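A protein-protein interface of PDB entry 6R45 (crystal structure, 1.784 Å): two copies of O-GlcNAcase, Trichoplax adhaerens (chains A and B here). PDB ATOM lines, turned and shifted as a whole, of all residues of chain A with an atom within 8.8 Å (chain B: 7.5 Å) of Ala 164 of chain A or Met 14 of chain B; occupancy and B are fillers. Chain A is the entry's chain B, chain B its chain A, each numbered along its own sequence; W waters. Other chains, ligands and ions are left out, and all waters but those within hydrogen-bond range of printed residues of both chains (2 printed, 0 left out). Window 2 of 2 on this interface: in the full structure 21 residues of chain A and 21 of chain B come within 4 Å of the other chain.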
ATOM      1  N   TYR A  63      -9.218   1.827  -7.533  1.00  0.00           N
ATOM      2  CA  TYR A  63      -8.837   2.446  -8.810  1.00  0.00           C
ATOM      3  C   TYR A  63      -7.350   2.725  -8.750  1.00  0.00           C
ATOM      4  O   TYR A  63      -6.828   3.175  -7.738  1.00  0.00           O
ATOM      5  CB  TYR A  63      -9.692   3.672  -9.082  1.00  0.00           C
ATOM      6  CG  TYR A  63     -10.976   3.253  -9.712  1.00  0.00           C
ATOM      7  CD1 TYR A  63     -12.027   2.784  -8.936  1.00  0.00           C
ATOM      8  CD2 TYR A  63     -11.150   3.368 -11.084  1.00  0.00           C
ATOM      9  CE1 TYR A  63     -13.232   2.420  -9.520  1.00  0.00           C
ATOM     10  CE2 TYR A  63     -12.350   3.019 -11.671  1.00  0.00           C
ATOM     11  CZ  TYR A  63     -13.378   2.521 -10.892  1.00  0.00           C
ATOM     12  OH  TYR A  63     -14.531   2.156 -11.526  1.00  0.00           O
ATOM     13  N   LEU A  80     -17.681   1.592  -0.336  1.00  0.00           N
ATOM     14  CA  LEU A  80     -19.118   1.972  -0.173  1.00  0.00           C
ATOM     15  C   LEU A  80     -19.631   1.786   1.264  1.00  0.00           C
ATOM     16  O   LEU A  80     -20.253   2.731   1.824  1.00  0.00           O
ATOM     17  CB  LEU A  80     -19.934   1.168  -1.175  1.00  0.00           C
ATOM     18  CG  LEU A  80     -21.414   1.537  -1.227  1.00  0.00           C
ATOM     19  CD1 LEU A  80     -21.566   3.003  -1.584  1.00  0.00           C
ATOM     20  CD2 LEU A  80     -22.126   0.663  -2.251  1.00  0.00           C
ATOM     21  N   SER A 136     -19.540   5.661   3.735  1.00  0.00           N
ATOM     22  CA  SER A 136     -18.415   5.178   2.903  1.00  0.00           C
ATOM     23  C   SER A 136     -17.099   5.676   3.490  1.00  0.00           C
ATOM     24  O   SER A 136     -17.085   6.564   4.349  1.00  0.00           O
ATOM     25  CB  SER A 136     -18.547   5.593   1.468  1.00  0.00           C
ATOM     26  OG  SER A 136     -19.817   5.252   0.942  1.00  0.00           O
ATOM     27  N   PHE A 157     -13.790  11.983  -8.854  1.00  0.00           N
ATOM     28  CA  PHE A 157     -14.304  10.736  -9.482  1.00  0.00           C
ATOM     29  C   PHE A 157     -14.849   9.760  -8.434  1.00  0.00           C
ATOM     30  O   PHE A 157     -16.003   9.245  -8.571  1.00  0.00           O
ATOM     31  CB  PHE A 157     -13.230  10.053 -10.340  1.00  0.00           C
ATOM     32  CG  PHE A 157     -13.598   8.631 -10.681  1.00  0.00           C
ATOM     33  CD1 PHE A 157     -14.738   8.376 -11.437  1.00  0.00           C
ATOM     34  CD2 PHE A 157     -12.875   7.550 -10.191  1.00  0.00           C
ATOM     35  CE1 PHE A 157     -15.138   7.082 -11.712  1.00  0.00           C
ATOM     36  CE2 PHE A 157     -13.290   6.251 -10.465  1.00  0.00           C
ATOM     37  CZ  PHE A 157     -14.410   6.023 -11.224  1.00  0.00           C
ATOM     38  N   ILE A 158     -14.039   9.432  -7.434  1.00  0.00           N
ATOM     39  CA  ILE A 158     -14.412   8.355  -6.481  1.00  0.00           C
ATOM     40  C   ILE A 158     -15.615   8.842  -5.667  1.00  0.00           C
ATOM     41  O   ILE A 158     -16.476   8.044  -5.422  1.00  0.00           O
ATOM     42  CB  ILE A 158     -13.246   7.898  -5.596  1.00  0.00           C
ATOM     43  CG1 ILE A 158     -13.558   6.521  -5.012  1.00  0.00           C
ATOM     44  CG2 ILE A 158     -12.924   8.926  -4.521  1.00  0.00           C
ATOM     45  CD1 ILE A 158     -13.866   5.486  -6.079  1.00  0.00           C
ATOM     46  N   LEU A 159     -15.712  10.132  -5.375  1.00  0.00           N
ATOM     47  CA  LEU A 159     -16.875  10.646  -4.601  1.00  0.00           C
ATOM     48  C   LEU A 159     -18.157  10.551  -5.451  1.00  0.00           C
ATOM     49  O   LEU A 159     -19.223  10.151  -4.901  1.00  0.00           O
ATOM     50  CB  LEU A 159     -16.579  12.073  -4.161  1.00  0.00           C
ATOM     51  CG  LEU A 159     -15.495  12.203  -3.087  1.00  0.00           C
ATOM     52  CD1 LEU A 159     -15.372  13.667  -2.694  1.00  0.00           C
ATOM     53  CD2 LEU A 159     -15.798  11.355  -1.864  1.00  0.00           C
ATOM     54  N   GLU A 160     -18.079  10.877  -6.743  1.00  0.00           N
ATOM     55  CA  GLU A 160     -19.236  10.712  -7.670  1.00  0.00           C
ATOM     56  C   GLU A 160     -19.626   9.226  -7.733  1.00  0.00           C
ATOM     57  O   GLU A 160     -20.856   8.915  -7.800  1.00  0.00           O
ATOM     58  CB  GLU A 160     -18.915  11.267  -9.063  1.00  0.00           C
ATOM     59  CG  GLU A 160     -19.060  12.782  -9.184  1.00  0.00           C
ATOM     60  CD  GLU A 160     -20.374  13.414  -8.737  1.00  0.00           C
ATOM     61  OE1 GLU A 160     -21.392  12.693  -8.569  1.00  0.00           O
ATOM     62  OE2 GLU A 160     -20.385  14.646  -8.571  1.00  0.00           O
ATOM     63  N   GLN A 161     -18.645   8.322  -7.772  1.00  0.00           N
ATOM     64  CA  GLN A 161     -18.918   6.859  -7.867  1.00  0.00           C
ATOM     65  C   GLN A 161     -19.681   6.410  -6.623  1.00  0.00           C
ATOM     66  O   GLN A 161     -20.665   5.642  -6.751  1.00  0.00           O
ATOM     67  CB  GLN A 161     -17.656   6.003  -7.994  1.00  0.00           C
ATOM     68  CG  GLN A 161     -17.118   5.926  -9.412  1.00  0.00           C
ATOM     69  CD  GLN A 161     -18.088   5.341 -10.417  1.00  0.00           C
ATOM     70  OE1 GLN A 161     -18.734   6.050 -11.194  1.00  0.00           O
ATOM     71  NE2 GLN A 161     -18.203   4.027 -10.399  1.00  0.00           N
ATOM     72  N   LEU A 162     -19.224   6.834  -5.445  1.00  0.00           N
ATOM     73  CA  LEU A 162     -19.897   6.449  -4.186  1.00  0.00           C
ATOM     74  C   LEU A 162     -21.298   7.049  -4.147  1.00  0.00           C
ATOM     75  O   LEU A 162     -22.224   6.309  -3.744  1.00  0.00           O
ATOM     76  CB  LEU A 162     -19.046   6.900  -3.005  1.00  0.00           C
ATOM     77  CG  LEU A 162     -17.733   6.135  -2.861  1.00  0.00           C
ATOM     78  CD1 LEU A 162     -16.818   6.828  -1.883  1.00  0.00           C
ATOM     79  CD2 LEU A 162     -17.973   4.699  -2.426  1.00  0.00           C
ATOM     80  N   LYS A 163     -21.454   8.321  -4.534  1.00  0.00           N
ATOM     81  CA  LYS A 163     -22.766   9.015  -4.439  1.00  0.00           C
ATOM     82  C   LYS A 163     -23.728   8.310  -5.384  1.00  0.00           C
ATOM     83  O   LYS A 163     -24.901   8.074  -5.005  1.00  0.00           O
ATOM     84  CB  LYS A 163     -22.608  10.491  -4.806  1.00  0.00           C
ATOM     85  CG  LYS A 163     -23.859  11.350  -4.743  1.00  0.00           C
ATOM     86  CD  LYS A 163     -23.656  12.685  -5.452  1.00  0.00           C
ATOM     87  CE  LYS A 163     -22.776  13.643  -4.677  1.00  0.00           C
ATOM     88  NZ  LYS A 163     -22.023  14.572  -5.553  1.00  0.00           N
ATOM     89  N   ALA A 164     -23.224   7.934  -6.561  1.00  0.00           N
ATOM     90  CA  ALA A 164     -24.011   7.229  -7.594  1.00  0.00           C
ATOM     91  C   ALA A 164     -24.448   5.864  -7.057  1.00  0.00           C
ATOM     92  O   ALA A 164     -25.479   5.381  -7.502  1.00  0.00           O
ATOM     93  CB  ALA A 164     -23.224   7.120  -8.872  1.00  0.00           C
ATOM     94  N   LYS A 165     -23.720   5.275  -6.109  1.00  0.00           N
ATOM     95  CA  LYS A 165     -24.072   3.973  -5.492  1.00  0.00           C
ATOM     96  C   LYS A 165     -24.909   4.192  -4.221  1.00  0.00           C
ATOM     97  O   LYS A 165     -25.065   3.224  -3.455  1.00  0.00           O
ATOM     98  CB  LYS A 165     -22.792   3.196  -5.187  1.00  0.00           C
ATOM     99  CG  LYS A 165     -21.983   2.868  -6.427  1.00  0.00           C
ATOM    100  CD  LYS A 165     -22.560   1.756  -7.236  1.00  0.00           C
ATOM    101  CE  LYS A 165     -21.719   0.502  -7.199  1.00  0.00           C
ATOM    102  NZ  LYS A 165     -22.454  -0.647  -7.769  1.00  0.00           N
ATOM    103  N   GLY A 166     -25.364   5.428  -3.987  1.00  0.00           N
ATOM    104  CA  GLY A 166     -26.257   5.811  -2.878  1.00  0.00           C
ATOM    105  C   GLY A 166     -25.519   6.238  -1.619  1.00  0.00           C
ATOM    106  O   GLY A 166     -26.161   6.369  -0.596  1.00  0.00           O
ATOM    107  N   SER A 167     -24.206   6.480  -1.658  1.00  0.00           N
ATOM    108  CA  SER A 167     -23.497   6.938  -0.439  1.00  0.00           C
ATOM    109  C   SER A 167     -23.975   8.354  -0.104  1.00  0.00           C
ATOM    110  O   SER A 167     -24.048   9.194  -0.996  1.00  0.00           O
ATOM    111  CB  SER A 167     -21.992   6.969  -0.592  1.00  0.00           C
ATOM    112  OG  SER A 167     -21.424   7.337   0.642  1.00  0.00           O
ATOM    113  N   TYR A 168     -24.174   8.623   1.164  1.00  0.00           N
ATOM    114  CA  TYR A 168     -24.538   9.965   1.658  1.00  0.00           C
ATOM    115  C   TYR A 168     -23.318  10.640   2.278  1.00  0.00           C
ATOM    116  O   TYR A 168     -23.453  11.751   2.804  1.00  0.00           O
ATOM    117  CB  TYR A 168     -25.731   9.847   2.617  1.00  0.00           C
ATOM    118  CG  TYR A 168     -25.632   8.779   3.679  1.00  0.00           C
ATOM    119  CD1 TYR A 168     -24.878   8.966   4.825  1.00  0.00           C
ATOM    120  CD2 TYR A 168     -26.305   7.573   3.526  1.00  0.00           C
ATOM    121  CE1 TYR A 168     -24.817   7.998   5.814  1.00  0.00           C
ATOM    122  CE2 TYR A 168     -26.268   6.597   4.500  1.00  0.00           C
ATOM    123  CZ  TYR A 168     -25.526   6.820   5.648  1.00  0.00           C
ATOM    124  OH  TYR A 168     -25.476   5.864   6.601  1.00  0.00           O
ATOM    125  N   LEU A 210     -22.097  13.490   0.924  1.00  0.00           N
ATOM    126  CA  LEU A 210     -22.084  12.741  -0.377  1.00  0.00           C
ATOM    127  C   LEU A 210     -20.680  12.301  -0.896  1.00  0.00           C
ATOM    128  O   LEU A 210     -19.923  13.063  -1.586  1.00  0.00           O
ATOM    129  CB  LEU A 210     -22.851  13.599  -1.384  1.00  0.00           C
ATOM    130  CG  LEU A 210     -24.220  14.087  -0.917  1.00  0.00           C
ATOM    131  CD1 LEU A 210     -25.164  14.321  -2.090  1.00  0.00           C
ATOM    132  CD2 LEU A 210     -24.847  13.111   0.046  1.00  0.00           C
ATOM    133  N   ARG B  11     -14.082   3.585 -16.613  1.00  0.00           N
ATOM    134  CA  ARG B  11     -14.827   3.036 -15.481  1.00  0.00           C
ATOM    135  C   ARG B  11     -16.021   2.294 -16.039  1.00  0.00           C
ATOM    136  O   ARG B  11     -16.454   2.551 -17.164  1.00  0.00           O
ATOM    137  CB  ARG B  11     -15.253   4.195 -14.579  1.00  0.00           C
ATOM    138  CG  ARG B  11     -16.030   5.269 -15.331  1.00  0.00           C
ATOM    139  CD  ARG B  11     -17.241   5.714 -14.583  1.00  0.00           C
ATOM    140  NE  ARG B  11     -17.876   6.856 -15.201  1.00  0.00           N
ATOM    141  CZ  ARG B  11     -19.056   6.810 -15.798  1.00  0.00           C
ATOM    142  NH1 ARG B  11     -19.699   5.654 -15.904  1.00  0.00           N
ATOM    143  NH2 ARG B  11     -19.576   7.920 -16.282  1.00  0.00           N
ATOM    144  N   PRO B  12     -16.586   1.372 -15.252  1.00  0.00           N
ATOM    145  CA  PRO B  12     -17.776   0.641 -15.681  1.00  0.00           C
ATOM    146  C   PRO B  12     -18.939   1.596 -15.955  1.00  0.00           C
ATOM    147  O   PRO B  12     -19.160   2.616 -15.274  1.00  0.00           O
ATOM    148  CB  PRO B  12     -18.073  -0.330 -14.533  1.00  0.00           C
ATOM    149  CG  PRO B  12     -16.750  -0.391 -13.766  1.00  0.00           C
ATOM    150  CD  PRO B  12     -16.148   0.991 -13.895  1.00  0.00           C
ATOM    151  N   PHE B  13     -19.710   1.206 -16.959  1.00  0.00           N
ATOM    152  CA  PHE B  13     -20.964   1.865 -17.345  1.00  0.00           C
ATOM    153  C   PHE B  13     -21.891   1.919 -16.128  1.00  0.00           C
ATOM    154  O   PHE B  13     -21.908   0.943 -15.338  1.00  0.00           O
ATOM    155  CB  PHE B  13     -21.630   1.041 -18.441  1.00  0.00           C
ATOM    156  CG  PHE B  13     -23.077   1.351 -18.702  1.00  0.00           C
ATOM    157  CD1 PHE B  13     -24.064   0.605 -18.087  1.00  0.00           C
ATOM    158  CD2 PHE B  13     -23.441   2.319 -19.625  1.00  0.00           C
ATOM    159  CE1 PHE B  13     -25.403   0.855 -18.356  1.00  0.00           C
ATOM    160  CE2 PHE B  13     -24.776   2.587 -19.886  1.00  0.00           C
ATOM    161  CZ  PHE B  13     -25.758   1.837 -19.262  1.00  0.00           C
ATOM    162  N   MET B  14     -22.608   3.024 -15.990  1.00  0.00           N
ATOM    163  CA  MET B  14     -23.775   3.143 -15.056  1.00  0.00           C
ATOM    164  C   MET B  14     -24.998   3.531 -15.883  1.00  0.00           C
ATOM    165  O   MET B  14     -24.885   4.317 -16.819  1.00  0.00           O
ATOM    166  CB  MET B  14     -23.541   4.232 -14.003  1.00  0.00           C
ATOM    167  CG  MET B  14     -22.117   4.310 -13.516  1.00  0.00           C
ATOM    168  SD  MET B  14     -21.838   5.661 -12.322  1.00  0.00           S
ATOM    169  CE  MET B  14     -22.345   7.114 -13.243  1.00  0.00           C
ATOM    170  N   PRO B  15     -26.218   3.023 -15.578  1.00  0.00           N
ATOM    171  CA  PRO B  15     -27.409   3.381 -16.358  1.00  0.00           C
ATOM    172  C   PRO B  15     -27.571   4.864 -16.685  1.00  0.00           C
ATOM    173  O   PRO B  15     -28.127   5.181 -17.721  1.00  0.00           O
ATOM    174  CB  PRO B  15     -28.552   2.921 -15.442  1.00  0.00           C
ATOM    175  CG  PRO B  15     -27.978   1.714 -14.754  1.00  0.00           C
ATOM    176  CD  PRO B  15     -26.518   2.052 -14.517  1.00  0.00           C
ATOM    177  N   SER B  16     -27.092   5.754 -15.807  1.00  0.00           N
ATOM    178  CA  SER B  16     -27.188   7.224 -15.999  1.00  0.00           C
ATOM    179  C   SER B  16     -26.365   7.666 -17.210  1.00  0.00           C
ATOM    180  O   SER B  16     -26.555   8.814 -17.697  1.00  0.00           O
ATOM    181  CB  SER B  16     -26.777   7.975 -14.742  1.00  0.00           C
ATOM    182  OG  SER B  16     -25.439   7.674 -14.379  1.00  0.00           O
ATOM    183  N   ASP B  17     -25.425   6.827 -17.667  1.00  0.00           N
ATOM    184  CA  ASP B  17     -24.563   7.186 -18.822  1.00  0.00           C
ATOM    185  C   ASP B  17     -25.308   7.086 -20.158  1.00  0.00           C
ATOM    186  O   ASP B  17     -24.798   7.620 -21.167  1.00  0.00           O
ATOM    187  CB  ASP B  17     -23.365   6.246 -18.903  1.00  0.00           C
ATOM    188  CG  ASP B  17     -22.477   6.288 -17.680  1.00  0.00           C
ATOM    189  OD1 ASP B  17     -22.337   7.379 -17.132  1.00  0.00           O
ATOM    190  OD2 ASP B  17     -21.875   5.228 -17.342  1.00  0.00           O
ATOM    191  N   GLU B  18     -26.439   6.384 -20.173  1.00  0.00           N
ATOM    192  CA  GLU B  18     -27.041   5.880 -21.425  1.00  0.00           C
ATOM    193  C   GLU B  18     -27.315   7.074 -22.327  1.00  0.00           C
ATOM    194  O   GLU B  18     -26.906   7.020 -23.469  1.00  0.00           O
ATOM    195  CB  GLU B  18     -28.273   5.028 -21.148  1.00  0.00           C
ATOM    196  CG  GLU B  18     -29.052   4.780 -22.408  1.00  0.00           C
ATOM    197  CD  GLU B  18     -30.220   3.823 -22.299  1.00  0.00           C
ATOM    198  OE1 GLU B  18     -30.147   2.849 -21.524  1.00  0.00           O
ATOM    199  OE2 GLU B  18     -31.208   4.070 -23.010  1.00  0.00           O
ATOM    200  N   GLU B  19     -27.907   8.159 -21.816  1.00  0.00           N
ATOM    201  CA  GLU B  19     -28.311   9.288 -22.680  1.00  0.00           C
ATOM    202  C   GLU B  19     -27.083   9.887 -23.357  1.00  0.00           C
ATOM    203  O   GLU B  19     -27.137  10.146 -24.585  1.00  0.00           O
ATOM    204  CB  GLU B  19     -29.077  10.352 -21.886  1.00  0.00           C
ATOM    205  CG  GLU B  19     -29.860  11.297 -22.781  1.00  0.00           C
ATOM    206  CD  GLU B  19     -30.331  12.601 -22.150  1.00  0.00           C
ATOM    207  OE1 GLU B  19     -30.547  12.643 -20.902  1.00  0.00           O
ATOM    208  OE2 GLU B  19     -30.474  13.584 -22.917  1.00  0.00           O
ATOM    209  N   LEU B  21     -24.121   8.529 -23.814  1.00  0.00           N
ATOM    210  CA  LEU B  21     -23.554   7.534 -24.748  1.00  0.00           C
ATOM    211  C   LEU B  21     -24.378   7.496 -26.028  1.00  0.00           C
ATOM    212  O   LEU B  21     -23.764   7.450 -27.080  1.00  0.00           O
ATOM    213  CB  LEU B  21     -23.510   6.171 -24.073  1.00  0.00           C
ATOM    214  CG  LEU B  21     -22.488   6.066 -22.956  1.00  0.00           C
ATOM    215  CD1 LEU B  21     -22.572   4.694 -22.303  1.00  0.00           C
ATOM    216  CD2 LEU B  21     -21.100   6.339 -23.520  1.00  0.00           C
ATOM    217  N   ILE B  55     -26.245  -2.894 -23.030  1.00  0.00           N
ATOM    218  CA  ILE B  55     -26.888  -2.279 -21.838  1.00  0.00           C
ATOM    219  C   ILE B  55     -27.910  -3.288 -21.313  1.00  0.00           C
ATOM    220  O   ILE B  55     -27.990  -3.489 -20.074  1.00  0.00           O
ATOM    221  CB  ILE B  55     -27.495  -0.921 -22.199  1.00  0.00           C
ATOM    222  CG1 ILE B  55     -26.386   0.060 -22.554  1.00  0.00           C
ATOM    223  CG2 ILE B  55     -28.419  -0.426 -21.084  1.00  0.00           C
ATOM    224  CD1 ILE B  55     -26.857   1.404 -23.009  1.00  0.00           C
ATOM    225  N   PRO B  59     -24.288  -5.132 -19.205  1.00  0.00           N
ATOM    226  CA  PRO B  59     -23.788  -3.783 -18.934  1.00  0.00           C
ATOM    227  C   PRO B  59     -22.379  -3.817 -18.339  1.00  0.00           C
ATOM    228  O   PRO B  59     -21.673  -2.846 -18.516  1.00  0.00           O
ATOM    229  CB  PRO B  59     -24.802  -3.166 -17.961  1.00  0.00           C
ATOM    230  CG  PRO B  59     -25.550  -4.355 -17.388  1.00  0.00           C
ATOM    231  CD  PRO B  59     -25.530  -5.419 -18.460  1.00  0.00           C
ATOM    232  N   ILE B  62     -19.350  -2.979 -20.551  1.00  0.00           N
ATOM    233  CA  ILE B  62     -19.242  -1.599 -21.092  1.00  0.00           C
ATOM    234  C   ILE B  62     -18.382  -0.770 -20.139  1.00  0.00           C
ATOM    235  O   ILE B  62     -18.694  -0.719 -18.954  1.00  0.00           O
ATOM    236  CB  ILE B  62     -20.618  -0.933 -21.210  1.00  0.00           C
ATOM    237  CG1 ILE B  62     -21.660  -1.805 -21.910  1.00  0.00           C
ATOM    238  CG2 ILE B  62     -20.461   0.427 -21.874  1.00  0.00           C
ATOM    239  CD1 ILE B  62     -23.038  -1.174 -21.897  1.00  0.00           C
ATOM    240  N   VAL B  64     -16.763   3.209 -19.822  1.00  0.00           N
ATOM    241  CA  VAL B  64     -16.986   4.602 -20.261  1.00  0.00           C
ATOM    242  C   VAL B  64     -15.729   5.410 -19.951  1.00  0.00           C
ATOM    243  O   VAL B  64     -15.161   5.253 -18.851  1.00  0.00           O
ATOM    244  CB  VAL B  64     -18.235   5.168 -19.576  1.00  0.00           C
ATOM    245  CG1 VAL B  64     -18.446   6.643 -19.897  1.00  0.00           C
ATOM    246  CG2 VAL B  64     -19.447   4.327 -19.928  1.00  0.00           C
ATOM    247  N   GLU B  66     -14.099   9.050 -19.289  1.00  0.00           N
ATOM    248  CA  GLU B  66     -14.296  10.468 -18.899  1.00  0.00           C
ATOM    249  C   GLU B  66     -12.998  11.251 -19.090  1.00  0.00           C
ATOM    250  O   GLU B  66     -11.927  10.715 -18.732  1.00  0.00           O
ATOM    251  CB  GLU B  66     -14.658  10.600 -17.426  1.00  0.00           C
ATOM    252  CG  GLU B  66     -15.992  10.013 -17.047  1.00  0.00           C
ATOM    253  CD  GLU B  66     -16.294  10.193 -15.567  1.00  0.00           C
ATOM    254  OE1 GLU B  66     -15.946  11.274 -15.057  1.00  0.00           O
ATOM    255  OE2 GLU B  66     -16.865   9.253 -14.935  1.00  0.00           O
ATOM    256  N   ILE B  72     -18.004  12.538 -20.725  1.00  0.00           N
ATOM    257  CA  ILE B  72     -17.955  11.211 -21.403  1.00  0.00           C
ATOM    258  C   ILE B  72     -17.512  11.448 -22.857  1.00  0.00           C
ATOM    259  O   ILE B  72     -18.206  12.152 -23.604  1.00  0.00           O
ATOM    260  CB  ILE B  72     -19.301  10.467 -21.282  1.00  0.00           C
ATOM    261  CG1 ILE B  72     -19.611  10.102 -19.830  1.00  0.00           C
ATOM    262  CG2 ILE B  72     -19.330   9.233 -22.167  1.00  0.00           C
ATOM    263  CD1 ILE B  72     -20.982   9.526 -19.607  1.00  0.00           C
HETATM  264  O   HOH W   1     -18.871   2.994 -12.749  1.00  0.00           O
HETATM  265  O   HOH W   2     -20.855   4.252  -9.330  1.00  0.00           O
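The side-chain sulfur (SD) of Met 14 of chain B lies close to the side-chain amide oxygen (OE1) of Gln 161 of chain A, 3.3 Å away.
The backbone NH (N) of Val 64 of chain B sits at hydrogen-bond distance from the backbone carbonyl oxygen (O) of Arg 11 of chain B, 2.8 Å away.
The backbone NH (N) of Met 14 of chain B sits at hydrogen-bond distance from the side-chain carboxylate (OD2) of Asp 17 of chain B, at 2.7 Å.
OE2 of Glu 66 of chain B is in salt-bridge range of NE of Arg 11 of chain B, at 2.6 Å.
The guanidinium group (NH1) of Arg 11 of chain B is in salt-bridge range of the side-chain carboxylate (OD2) of Asp 17 of chain B, at 2.6 Å.
OH of Tyr 63 of chain A touches CB of Arg 11 of chain B, at 3.7 Å.
CD of Pro 12 of chain B touches OH of Tyr 63 of chain A, at 3.1 Å.
Phe 157 of chain A touches Arg 11 of chain B.
Arg 11 of chain B touches Gln 161 of chain A (CD to OE1, 3.7 Å).
Ala 164 of chain A touches Met 14 of chain B (CB to SD, 3.99 Å).
Of the printed residues of chain B, Tyr 63 of chain A touches Arg 11 (3.7 Å) and Pro 12 (3.1 Å).
Printed residues of chain B within 4 Å of Phe 157 of chain A: Arg 11.
Printed residues of chain B within 4 Å of Gln 161 of chain A: Arg 11 and Met 14.
Of the printed residues of chain B, Ala 164 of chain A touches Met 14.
Ser 167 of chain A touches none of the printed residues of chain B.
Printed residues of chain A within 4 Å of Pro 12 of chain B: Tyr 63.
Of the printed residues of chain A, Met 14 of chain B touches Gln 161 (3.3 Å) and Ala 164 (3.99 Å).
Pro 15 of chain B touches none of the printed residues of chain A.
Asp 17 of chain B touches none of the printed residues of chain A.
The nearest printed residue of chain B that does not touch Ala 164 of chain A is Ser 16 of chain B (6.0 Å).
The nearest printed residue of chain A that does not touch Met 14 of chain B is Glu 160 of chain A (5.7 Å).
The nearest printed residue of chain B that does not touch Tyr 63 of chain A is Phe 13 of chain B (7.6 Å).
Of the 16 printed residues of chain A, 4 touch a printed residue of chain B.
Hydrophobic or aromatic side chains of chain A within 4 Å of the printed part of chain B: Tyr 63, Phe 157 and Ala 164.
Among the printed residues, no Asp or Glu carboxylate lies within 4 Å of a Lys or Arg side-chain nitrogen of the other chain.
No position is printed for both chains.
Water W1 bridges O of Pro 12 of chain B (2.6 Å) and NE2 of Gln 161 of chain A (2.7 Å).
Water W2 lies within hydrogen-bond range of NE2 of Gln 161 of chain A (2.9 Å) and SD of Met 14 of chain B (3.5 Å).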
